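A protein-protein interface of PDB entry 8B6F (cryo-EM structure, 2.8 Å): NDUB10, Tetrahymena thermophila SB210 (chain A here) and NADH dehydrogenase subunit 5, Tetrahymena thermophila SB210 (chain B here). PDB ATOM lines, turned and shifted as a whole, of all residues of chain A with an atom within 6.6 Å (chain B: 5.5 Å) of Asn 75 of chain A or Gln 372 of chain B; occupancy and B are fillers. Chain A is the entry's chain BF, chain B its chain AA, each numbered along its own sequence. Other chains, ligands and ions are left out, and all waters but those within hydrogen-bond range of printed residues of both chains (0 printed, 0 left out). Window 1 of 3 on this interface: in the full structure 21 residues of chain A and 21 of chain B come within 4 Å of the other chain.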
ATOM      1  N   ASN A  68     -29.488 -21.664  32.443  1.00  0.00           N
ATOM      2  CA  ASN A  68     -28.573 -20.533  32.553  1.00  0.00           C
ATOM      3  C   ASN A  68     -27.437 -20.662  31.548  1.00  0.00           C
ATOM      4  O   ASN A  68     -26.962 -19.660  31.003  1.00  0.00           O
ATOM      5  CB  ASN A  68     -28.021 -20.427  33.973  1.00  0.00           C
ATOM      6  CG  ASN A  68     -29.061 -19.961  34.969  1.00  0.00           C
ATOM      7  OD1 ASN A  68     -30.050 -19.332  34.601  1.00  0.00           O
ATOM      8  ND2 ASN A  68     -28.836 -20.261  36.241  1.00  0.00           N
ATOM      9  N   TYR A  70     -27.703 -22.128  28.597  1.00  0.00           N
ATOM     10  CA  TYR A  70     -28.291 -21.703  27.331  1.00  0.00           C
ATOM     11  C   TYR A  70     -28.241 -20.188  27.195  1.00  0.00           C
ATOM     12  O   TYR A  70     -27.873 -19.659  26.140  1.00  0.00           O
ATOM     13  CB  TYR A  70     -29.738 -22.192  27.229  1.00  0.00           C
ATOM     14  CG  TYR A  70     -29.911 -23.617  26.748  1.00  0.00           C
ATOM     15  CD1 TYR A  70     -28.817 -24.417  26.460  1.00  0.00           C
ATOM     16  CD2 TYR A  70     -31.178 -24.150  26.555  1.00  0.00           C
ATOM     17  CE1 TYR A  70     -28.975 -25.703  26.015  1.00  0.00           C
ATOM     18  CE2 TYR A  70     -31.346 -25.445  26.106  1.00  0.00           C
ATOM     19  CZ  TYR A  70     -30.234 -26.214  25.836  1.00  0.00           C
ATOM     20  OH  TYR A  70     -30.344 -27.508  25.388  1.00  0.00           O
ATOM     21  N   ARG A  71     -28.617 -19.468  28.253  1.00  0.00           N
ATOM     22  CA  ARG A  71     -28.596 -18.012  28.193  1.00  0.00           C
ATOM     23  C   ARG A  71     -27.177 -17.494  27.987  1.00  0.00           C
ATOM     24  O   ARG A  71     -26.954 -16.558  27.212  1.00  0.00           O
ATOM     25  CB  ARG A  71     -29.204 -17.426  29.466  1.00  0.00           C
ATOM     26  CG  ARG A  71     -29.505 -15.938  29.382  1.00  0.00           C
ATOM     27  CD  ARG A  71     -30.544 -15.660  28.307  1.00  0.00           C
ATOM     28  NE  ARG A  71     -31.060 -14.298  28.363  1.00  0.00           N
ATOM     29  CZ  ARG A  71     -30.561 -13.272  27.690  1.00  0.00           C
ATOM     30  NH1 ARG A  71     -29.510 -13.407  26.900  1.00  0.00           N
ATOM     31  NH2 ARG A  71     -31.133 -12.078  27.811  1.00  0.00           N
ATOM     32  N   LYS A  72     -26.210 -18.066  28.704  1.00  0.00           N
ATOM     33  CA  LYS A  72     -24.824 -17.643  28.542  1.00  0.00           C
ATOM     34  C   LYS A  72     -24.327 -17.919  27.129  1.00  0.00           C
ATOM     35  O   LYS A  72     -23.614 -17.099  26.541  1.00  0.00           O
ATOM     36  CB  LYS A  72     -23.940 -18.348  29.568  1.00  0.00           C
ATOM     37  CG  LYS A  72     -24.260 -17.981  31.005  1.00  0.00           C
ATOM     38  CD  LYS A  72     -23.784 -19.048  31.976  1.00  0.00           C
ATOM     39  CE  LYS A  72     -22.283 -19.255  31.891  1.00  0.00           C
ATOM     40  NZ  LYS A  72     -21.817 -20.284  32.857  1.00  0.00           N
ATOM     41  N   ARG A  73     -24.688 -19.076  26.571  1.00  0.00           N
ATOM     42  CA  ARG A  73     -24.256 -19.411  25.220  1.00  0.00           C
ATOM     43  C   ARG A  73     -24.846 -18.458  24.188  1.00  0.00           C
ATOM     44  O   ARG A  73     -24.147 -18.024  23.266  1.00  0.00           O
ATOM     45  CB  ARG A  73     -24.645 -20.852  24.892  1.00  0.00           C
ATOM     46  CG  ARG A  73     -23.942 -21.889  25.749  1.00  0.00           C
ATOM     47  CD  ARG A  73     -22.525 -22.147  25.275  1.00  0.00           C
ATOM     48  NE  ARG A  73     -21.856 -23.131  26.117  1.00  0.00           N
ATOM     49  CZ  ARG A  73     -20.666 -23.656  25.862  1.00  0.00           C
ATOM     50  NH1 ARG A  73     -19.977 -23.316  24.785  1.00  0.00           N
ATOM     51  NH2 ARG A  73     -20.155 -24.546  26.708  1.00  0.00           N
ATOM     52  N   ILE A  74     -26.126 -18.112  24.325  1.00  0.00           N
ATOM     53  CA  ILE A  74     -26.738 -17.204  23.360  1.00  0.00           C
ATOM     54  C   ILE A  74     -26.141 -15.808  23.492  1.00  0.00           C
ATOM     55  O   ILE A  74     -25.953 -15.106  22.493  1.00  0.00           O
ATOM     56  CB  ILE A  74     -28.272 -17.199  23.513  1.00  0.00           C
ATOM     57  CG1 ILE A  74     -28.940 -16.514  22.319  1.00  0.00           C
ATOM     58  CG2 ILE A  74     -28.704 -16.514  24.789  1.00  0.00           C
ATOM     59  CD1 ILE A  74     -28.827 -17.299  21.032  1.00  0.00           C
ATOM     60  N   ASN A  75     -25.818 -15.387  24.717  1.00  0.00           N
ATOM     61  CA  ASN A  75     -25.139 -14.108  24.898  1.00  0.00           C
ATOM     62  C   ASN A  75     -23.768 -14.117  24.235  1.00  0.00           C
ATOM     63  O   ASN A  75     -23.374 -13.138  23.592  1.00  0.00           O
ATOM     64  CB  ASN A  75     -25.010 -13.779  26.385  1.00  0.00           C
ATOM     65  CG  ASN A  75     -26.324 -13.359  27.008  1.00  0.00           C
ATOM     66  OD1 ASN A  75     -27.099 -12.620  26.405  1.00  0.00           O
ATOM     67  ND2 ASN A  75     -26.577 -13.819  28.226  1.00  0.00           N
ATOM     68  N   ASN A  76     -23.024 -15.214  24.387  1.00  0.00           N
ATOM     69  CA  ASN A  76     -21.721 -15.322  23.739  1.00  0.00           C
ATOM     70  C   ASN A  76     -21.859 -15.295  22.224  1.00  0.00           C
ATOM     71  O   ASN A  76     -21.027 -14.702  21.527  1.00  0.00           O
ATOM     72  CB  ASN A  76     -21.012 -16.598  24.191  1.00  0.00           C
ATOM     73  CG  ASN A  76     -20.753 -16.625  25.681  1.00  0.00           C
ATOM     74  OD1 ASN A  76     -20.616 -15.581  26.316  1.00  0.00           O
ATOM     75  ND2 ASN A  76     -20.675 -17.823  26.246  1.00  0.00           N
ATOM     76  N   GLU A  77     -22.897 -15.941  21.694  1.00  0.00           N
ATOM     77  CA  GLU A  77     -23.136 -15.909  20.255  1.00  0.00           C
ATOM     78  C   GLU A  77     -23.466 -14.498  19.784  1.00  0.00           C
ATOM     79  O   GLU A  77     -23.070 -14.096  18.684  1.00  0.00           O
ATOM     80  CB  GLU A  77     -24.262 -16.876  19.891  1.00  0.00           C
ATOM     81  CG  GLU A  77     -23.900 -18.339  20.090  1.00  0.00           C
ATOM     82  CD  GLU A  77     -22.785 -18.796  19.170  1.00  0.00           C
ATOM     83  OE1 GLU A  77     -22.458 -18.059  18.218  1.00  0.00           O
ATOM     84  OE2 GLU A  77     -22.233 -19.891  19.401  1.00  0.00           O
ATOM     85  N   VAL A  78     -24.199 -13.733  20.594  1.00  0.00           N
ATOM     86  CA  VAL A  78     -24.482 -12.345  20.238  1.00  0.00           C
ATOM     87  C   VAL A  78     -23.196 -11.532  20.202  1.00  0.00           C
ATOM     88  O   VAL A  78     -22.998 -10.693  19.316  1.00  0.00           O
ATOM     89  CB  VAL A  78     -25.500 -11.739  21.221  1.00  0.00           C
ATOM     90  CG1 VAL A  78     -25.649 -10.240  20.998  1.00  0.00           C
ATOM     91  CG2 VAL A  78     -26.830 -12.410  21.070  1.00  0.00           C
ATOM     92  N   ARG A  79     -22.307 -11.753  21.172  1.00  0.00           N
ATOM     93  CA  ARG A  79     -21.015 -11.076  21.145  1.00  0.00           C
ATOM     94  C   ARG A  79     -20.229 -11.461  19.900  1.00  0.00           C
ATOM     95  O   ARG A  79     -19.604 -10.609  19.261  1.00  0.00           O
ATOM     96  CB  ARG A  79     -20.222 -11.409  22.407  1.00  0.00           C
ATOM     97  CG  ARG A  79     -18.795 -10.884  22.396  1.00  0.00           C
ATOM     98  CD  ARG A  79     -18.079 -11.227  23.687  1.00  0.00           C
ATOM     99  NE  ARG A  79     -17.989 -12.666  23.898  1.00  0.00           N
ATOM    100  CZ  ARG A  79     -17.649 -13.235  25.046  1.00  0.00           C
ATOM    101  NH1 ARG A  79     -17.368 -12.515  26.119  1.00  0.00           N
ATOM    102  NH2 ARG A  79     -17.590 -14.562  25.119  1.00  0.00           N
ATOM    103  N   ARG A  80     -20.238 -12.749  19.549  1.00  0.00           N
ATOM    104  CA  ARG A  80     -19.546 -13.195  18.346  1.00  0.00           C
ATOM    105  C   ARG A  80     -20.125 -12.526  17.107  1.00  0.00           C
ATOM    106  O   ARG A  80     -19.381 -12.082  16.226  1.00  0.00           O
ATOM    107  CB  ARG A  80     -19.638 -14.717  18.233  1.00  0.00           C
ATOM    108  CG  ARG A  80     -19.129 -15.292  16.919  1.00  0.00           C
ATOM    109  CD  ARG A  80     -19.425 -16.776  16.834  1.00  0.00           C
ATOM    110  NE  ARG A  80     -18.653 -17.538  17.808  1.00  0.00           N
ATOM    111  CZ  ARG A  80     -17.472 -18.092  17.571  1.00  0.00           C
ATOM    112  NH1 ARG A  80     -16.887 -18.000  16.389  1.00  0.00           N
ATOM    113  NH2 ARG A  80     -16.866 -18.765  18.544  1.00  0.00           N
ATOM    114  N   MET A  94     -29.680 -10.287  13.150  1.00  0.00           N
ATOM    115  CA  MET A  94     -30.111 -10.662  14.490  1.00  0.00           C
ATOM    116  C   MET A  94     -31.618 -10.847  14.578  1.00  0.00           C
ATOM    117  O   MET A  94     -32.089 -11.635  15.403  1.00  0.00           O
ATOM    118  CB  MET A  94     -29.665  -9.614  15.511  1.00  0.00           C
ATOM    119  CG  MET A  94     -28.199  -9.710  15.891  1.00  0.00           C
ATOM    120  SD  MET A  94     -27.753  -8.611  17.250  1.00  0.00           S
ATOM    121  CE  MET A  94     -28.751  -9.277  18.583  1.00  0.00           C
ATOM    122  N   ILE A 102     -33.153 -15.172  22.371  1.00  0.00           N
ATOM    123  CA  ILE A 102     -32.758 -14.272  23.452  1.00  0.00           C
ATOM    124  C   ILE A 102     -33.971 -13.898  24.293  1.00  0.00           C
ATOM    125  O   ILE A 102     -33.929 -13.930  25.528  1.00  0.00           O
ATOM    126  CB  ILE A 102     -32.083 -13.020  22.867  1.00  0.00           C
ATOM    127  CG1 ILE A 102     -30.735 -13.389  22.258  1.00  0.00           C
ATOM    128  CG2 ILE A 102     -31.898 -11.950  23.939  1.00  0.00           C
ATOM    129  CD1 ILE A 102     -30.172 -12.312  21.376  1.00  0.00           C
ATOM    130  N   THR B 361     -30.703  -9.076  31.672  1.00  0.00           N
ATOM    131  CA  THR B 361     -29.986  -9.989  30.796  1.00  0.00           C
ATOM    132  C   THR B 361     -28.884 -10.662  31.598  1.00  0.00           C
ATOM    133  O   THR B 361     -28.117  -9.988  32.292  1.00  0.00           O
ATOM    134  CB  THR B 361     -29.388  -9.253  29.595  1.00  0.00           C
ATOM    135  OG1 THR B 361     -28.311  -8.414  30.032  1.00  0.00           O
ATOM    136  CG2 THR B 361     -30.439  -8.396  28.915  1.00  0.00           C
ATOM    137  N   TYR B 362     -28.799 -11.986  31.492  1.00  0.00           N
ATOM    138  CA  TYR B 362     -27.832 -12.770  32.256  1.00  0.00           C
ATOM    139  C   TYR B 362     -26.450 -12.674  31.607  1.00  0.00           C
ATOM    140  O   TYR B 362     -25.812 -13.666  31.259  1.00  0.00           O
ATOM    141  CB  TYR B 362     -28.315 -14.212  32.347  1.00  0.00           C
ATOM    142  CG  TYR B 362     -27.555 -15.086  33.312  1.00  0.00           C
ATOM    143  CD1 TYR B 362     -27.299 -14.671  34.611  1.00  0.00           C
ATOM    144  CD2 TYR B 362     -27.135 -16.352  32.935  1.00  0.00           C
ATOM    145  CE1 TYR B 362     -26.620 -15.482  35.495  1.00  0.00           C
ATOM    146  CE2 TYR B 362     -26.455 -17.167  33.809  1.00  0.00           C
ATOM    147  CZ  TYR B 362     -26.201 -16.729  35.088  1.00  0.00           C
ATOM    148  OH  TYR B 362     -25.529 -17.547  35.961  1.00  0.00           O
ATOM    149  N   ASN B 363     -25.988 -11.436  31.456  1.00  0.00           N
ATOM    150  CA  ASN B 363     -24.755 -11.166  30.735  1.00  0.00           C
ATOM    151  C   ASN B 363     -24.214  -9.808  31.147  1.00  0.00           C
ATOM    152  O   ASN B 363     -24.977  -8.880  31.427  1.00  0.00           O
ATOM    153  CB  ASN B 363     -24.989 -11.215  29.221  1.00  0.00           C
ATOM    154  CG  ASN B 363     -24.060 -10.300  28.456  1.00  0.00           C
ATOM    155  OD1 ASN B 363     -22.945 -10.682  28.105  1.00  0.00           O
ATOM    156  ND2 ASN B 363     -24.516  -9.081  28.193  1.00  0.00           N
ATOM    157  N   LEU B 367     -20.563  -5.527  24.413  1.00  0.00           N
ATOM    158  CA  LEU B 367     -21.107  -5.679  23.067  1.00  0.00           C
ATOM    159  C   LEU B 367     -22.453  -6.383  23.094  1.00  0.00           C
ATOM    160  O   LEU B 367     -23.388  -5.982  22.393  1.00  0.00           O
ATOM    161  CB  LEU B 367     -20.127  -6.447  22.181  1.00  0.00           C
ATOM    162  CG  LEU B 367     -19.038  -5.613  21.508  1.00  0.00           C
ATOM    163  CD1 LEU B 367     -18.191  -4.898  22.533  1.00  0.00           C
ATOM    164  CD2 LEU B 367     -18.174  -6.487  20.621  1.00  0.00           C
ATOM    165  N   SER B 368     -22.569  -7.445  23.888  1.00  0.00           N
ATOM    166  CA  SER B 368     -23.835  -8.162  23.971  1.00  0.00           C
ATOM    167  C   SER B 368     -24.936  -7.265  24.522  1.00  0.00           C
ATOM    168  O   SER B 368     -26.062  -7.269  24.013  1.00  0.00           O
ATOM    169  CB  SER B 368     -23.668  -9.407  24.839  1.00  0.00           C
ATOM    170  OG  SER B 368     -24.863 -10.166  24.878  1.00  0.00           O
ATOM    171  N   PHE B 369     -24.631  -6.486  25.561  1.00  0.00           N
ATOM    172  CA  PHE B 369     -25.625  -5.570  26.112  1.00  0.00           C
ATOM    173  C   PHE B 369     -26.040  -4.522  25.088  1.00  0.00           C
ATOM    174  O   PHE B 369     -27.230  -4.220  24.946  1.00  0.00           O
ATOM    175  CB  PHE B 369     -25.080  -4.899  27.370  1.00  0.00           C
ATOM    176  CG  PHE B 369     -25.934  -3.773  27.872  1.00  0.00           C
ATOM    177  CD1 PHE B 369     -27.064  -4.031  28.627  1.00  0.00           C
ATOM    178  CD2 PHE B 369     -25.610  -2.456  27.588  1.00  0.00           C
ATOM    179  CE1 PHE B 369     -27.852  -3.001  29.092  1.00  0.00           C
ATOM    180  CE2 PHE B 369     -26.397  -1.421  28.051  1.00  0.00           C
ATOM    181  CZ  PHE B 369     -27.519  -1.694  28.803  1.00  0.00           C
ATOM    182  N   ASN B 370     -25.074  -3.956  24.364  1.00  0.00           N
ATOM    183  CA  ASN B 370     -25.401  -2.930  23.379  1.00  0.00           C
ATOM    184  C   ASN B 370     -26.296  -3.482  22.278  1.00  0.00           C
ATOM    185  O   ASN B 370     -27.216  -2.799  21.815  1.00  0.00           O
ATOM    186  CB  ASN B 370     -24.119  -2.353  22.780  1.00  0.00           C
ATOM    187  CG  ASN B 370     -23.355  -1.487  23.758  1.00  0.00           C
ATOM    188  OD1 ASN B 370     -23.615  -1.511  24.959  1.00  0.00           O
ATOM    189  ND2 ASN B 370     -22.407  -0.711  23.247  1.00  0.00           N
ATOM    190  N   ASN B 371     -26.044  -4.714  21.844  1.00  0.00           N
ATOM    191  CA  ASN B 371     -26.821  -5.322  20.775  1.00  0.00           C
ATOM    192  C   ASN B 371     -28.094  -6.003  21.258  1.00  0.00           C
ATOM    193  O   ASN B 371     -28.891  -6.442  20.424  1.00  0.00           O
ATOM    194  CB  ASN B 371     -25.957  -6.336  20.020  1.00  0.00           C
ATOM    195  CG  ASN B 371     -24.771  -5.689  19.337  1.00  0.00           C
ATOM    196  OD1 ASN B 371     -23.621  -5.989  19.646  1.00  0.00           O
ATOM    197  ND2 ASN B 371     -25.047  -4.789  18.402  1.00  0.00           N
ATOM    198  N   GLN B 372     -28.308  -6.109  22.572  1.00  0.00           N
ATOM    199  CA  GLN B 372     -29.516  -6.715  23.114  1.00  0.00           C
ATOM    200  C   GLN B 372     -30.497  -5.726  23.721  1.00  0.00           C
ATOM    201  O   GLN B 372     -31.678  -6.057  23.847  1.00  0.00           O
ATOM    202  CB  GLN B 372     -29.163  -7.744  24.197  1.00  0.00           C
ATOM    203  CG  GLN B 372     -28.578  -9.038  23.683  1.00  0.00           C
ATOM    204  CD  GLN B 372     -28.334 -10.029  24.799  1.00  0.00           C
ATOM    205  OE1 GLN B 372     -28.505  -9.710  25.974  1.00  0.00           O
ATOM    206  NE2 GLN B 372     -27.939 -11.243  24.438  1.00  0.00           N
ATOM    207  N   ILE B 373     -30.042  -4.532  24.107  1.00  0.00           N
ATOM    208  CA  ILE B 373     -30.888  -3.641  24.894  1.00  0.00           C
ATOM    209  C   ILE B 373     -32.174  -3.289  24.157  1.00  0.00           C
ATOM    210  O   ILE B 373     -33.205  -3.028  24.788  1.00  0.00           O
ATOM    211  CB  ILE B 373     -30.093  -2.379  25.286  1.00  0.00           C
ATOM    212  CG1 ILE B 373     -30.868  -1.543  26.311  1.00  0.00           C
ATOM    213  CG2 ILE B 373     -29.771  -1.540  24.060  1.00  0.00           C
ATOM    214  CD1 ILE B 373     -31.123  -2.261  27.628  1.00  0.00           C
ATOM    215  N   TYR B 374     -32.144  -3.273  22.824  1.00  0.00           N
ATOM    216  CA  TYR B 374     -33.335  -2.888  22.072  1.00  0.00           C
ATOM    217  C   TYR B 374     -34.473  -3.881  22.269  1.00  0.00           C
ATOM    218  O   TYR B 374     -35.644  -3.485  22.279  1.00  0.00           O
ATOM    219  CB  TYR B 374     -33.002  -2.741  20.588  1.00  0.00           C
ATOM    220  CG  TYR B 374     -32.869  -4.044  19.838  1.00  0.00           C
ATOM    221  CD1 TYR B 374     -31.744  -4.844  19.986  1.00  0.00           C
ATOM    222  CD2 TYR B 374     -33.861  -4.462  18.964  1.00  0.00           C
ATOM    223  CE1 TYR B 374     -31.620  -6.031  19.294  1.00  0.00           C
ATOM    224  CE2 TYR B 374     -33.745  -5.647  18.269  1.00  0.00           C
ATOM    225  CZ  TYR B 374     -32.623  -6.426  18.438  1.00  0.00           C
ATOM    226  OH  TYR B 374     -32.503  -7.608  17.746  1.00  0.00           O
ATOM    227  N   LEU B 375     -34.157  -5.168  22.423  1.00  0.00           N
ATOM    228  CA  LEU B 375     -35.199  -6.161  22.656  1.00  0.00           C
ATOM    229  C   LEU B 375     -35.936  -5.897  23.961  1.00  0.00           C
ATOM    230  O   LEU B 375     -37.169  -5.985  24.015  1.00  0.00           O
ATOM    231  CB  LEU B 375     -34.589  -7.562  22.670  1.00  0.00           C
ATOM    232  CG  LEU B 375     -33.945  -8.035  21.369  1.00  0.00           C
ATOM    233  CD1 LEU B 375     -33.237  -9.361  21.584  1.00  0.00           C
ATOM    234  CD2 LEU B 375     -34.983  -8.156  20.271  1.00  0.00           C
ATOM    235  N   TYR B 376     -35.205  -5.569  25.019  1.00  0.00           N
ATOM    236  CA  TYR B 376     -35.782  -5.339  26.335  1.00  0.00           C
ATOM    237  C   TYR B 376     -36.250  -3.906  26.538  1.00  0.00           C
ATOM    238  O   TYR B 376     -36.744  -3.580  27.621  1.00  0.00           O
ATOM    239  CB  TYR B 376     -34.766  -5.704  27.423  1.00  0.00           C
ATOM    240  CG  TYR B 376     -34.394  -7.168  27.436  1.00  0.00           C
ATOM    241  CD1 TYR B 376     -33.387  -7.656  26.614  1.00  0.00           C
ATOM    242  CD2 TYR B 376     -35.053  -8.061  28.267  1.00  0.00           C
ATOM    243  CE1 TYR B 376     -33.048  -8.995  26.621  1.00  0.00           C
ATOM    244  CE2 TYR B 376     -34.721  -9.400  28.282  1.00  0.00           C
ATOM    245  CZ  TYR B 376     -33.717  -9.861  27.457  1.00  0.00           C
ATOM    246  OH  TYR B 376     -33.385 -11.196  27.472  1.00  0.00           O
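The backbone carbonyl oxygen (O) of Lys 72 of chain A lies close to the side-chain amide nitrogen (ND2) of Asn 76 of chain A (3.0 Å). NH1 of Arg 71 of chain A sits at hydrogen-bond distance from OD1 of Asn 75 of chain A (2.6 Å). NE2 of Gln 372 of chain B sits at hydrogen-bond distance from OG of Ser 368 of chain B. O of Leu 367 of chain B sits close to OD1 of Asn 371 of chain B, 2.8 Å away.
Arg 71 of chain A touches Thr 361 of chain B. Tyr 362 of chain B touches Arg 71 of chain A (CB to CG, 3.6 Å). Gln 372 of chain B touches Arg 71 of chain A. Tyr 362 of chain B touches Lys 72 of chain A (CE2 to CG, 3.7 Å). Asn 75 of chain A touches Asn 363 of chain B. OG of Ser 368 of chain B touches O of Asn 75 of chain A, at 3.6 Å. Ser 368 of chain B touches Val 78 of chain A. CG2 of Val 78 of chain A touches NE2 of Gln 372 of chain B (3.7 Å). Met 94 of chain A touches Asn 371 of chain B (CE to O, 3.4 Å). Leu 375 of chain B touches Ile 102 of chain A (CD1 to CG2, 3.7 Å).
The side-chain hydroxyl (OH) of Tyr 376 of chain B lies within hydrogen-bond range of the guanidinium group (NH2) of Arg 71 of chain A, at 2.4 Å. The side-chain amide nitrogen (ND2) of Asn 75 of chain A lies within hydrogen-bond range of the backbone carbonyl oxygen (O) of Tyr 362 of chain B (3.1 Å). The side-chain amide nitrogen (NE2) of Gln 372 of chain B sits at hydrogen-bond distance from the side-chain amide oxygen (OD1) of Asn 75 of chain A. The backbone carbonyl oxygen (O) of Ile 102 of chain A sits at hydrogen-bond distance from the side-chain hydroxyl (OH) of Tyr 376 of chain B.
Hydrophobic or aromatic side chains of chain B that line the printed part of chain A: Tyr 362, Leu 375 and Tyr 376. Of the 14 printed residues of chain A, 7 touch a printed residue of chain B. Among the printed residues, no Asp or Glu carboxylate lies within 4 Å of a Lys or Arg side-chain nitrogen of the other chain.
Printed residues of chain B within 4 Å of Asn 68 of chain A: Tyr 362. Of the printed residues of chain B, Arg 71 of chain A touches Thr 361 (3.8 Å), Tyr 362 (3.6 Å), Gln 372 (3.6 Å) and Tyr 376 (2.4 Å). Asn 75 of chain A touches just these residues of chain B: Tyr 362, Asn 363, Ser 368 and Gln 372. Printed residues of chain B within 4 Å of Val 78 of chain A: Ser 368 and Gln 372. Of the printed residues of chain B, Met 94 of chain A touches Asn 371. Of the printed residues of chain A, Asn 363 of chain B touches Asn 75. Gln 372 of chain B touches just these residues of chain A: Arg 71 (3.6 Å), Asn 75 (2.5 Å), Val 78 (3.7 Å) and Ile 102 (3.9 Å). The nearest residue of chain A that does not touch Gln 372 of chain B is Ile 74 of chain A (4.8 Å). The nearest printed residue of chain A that does not touch Asn 363 of chain B is Arg 71 of chain A (5.5 Å).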
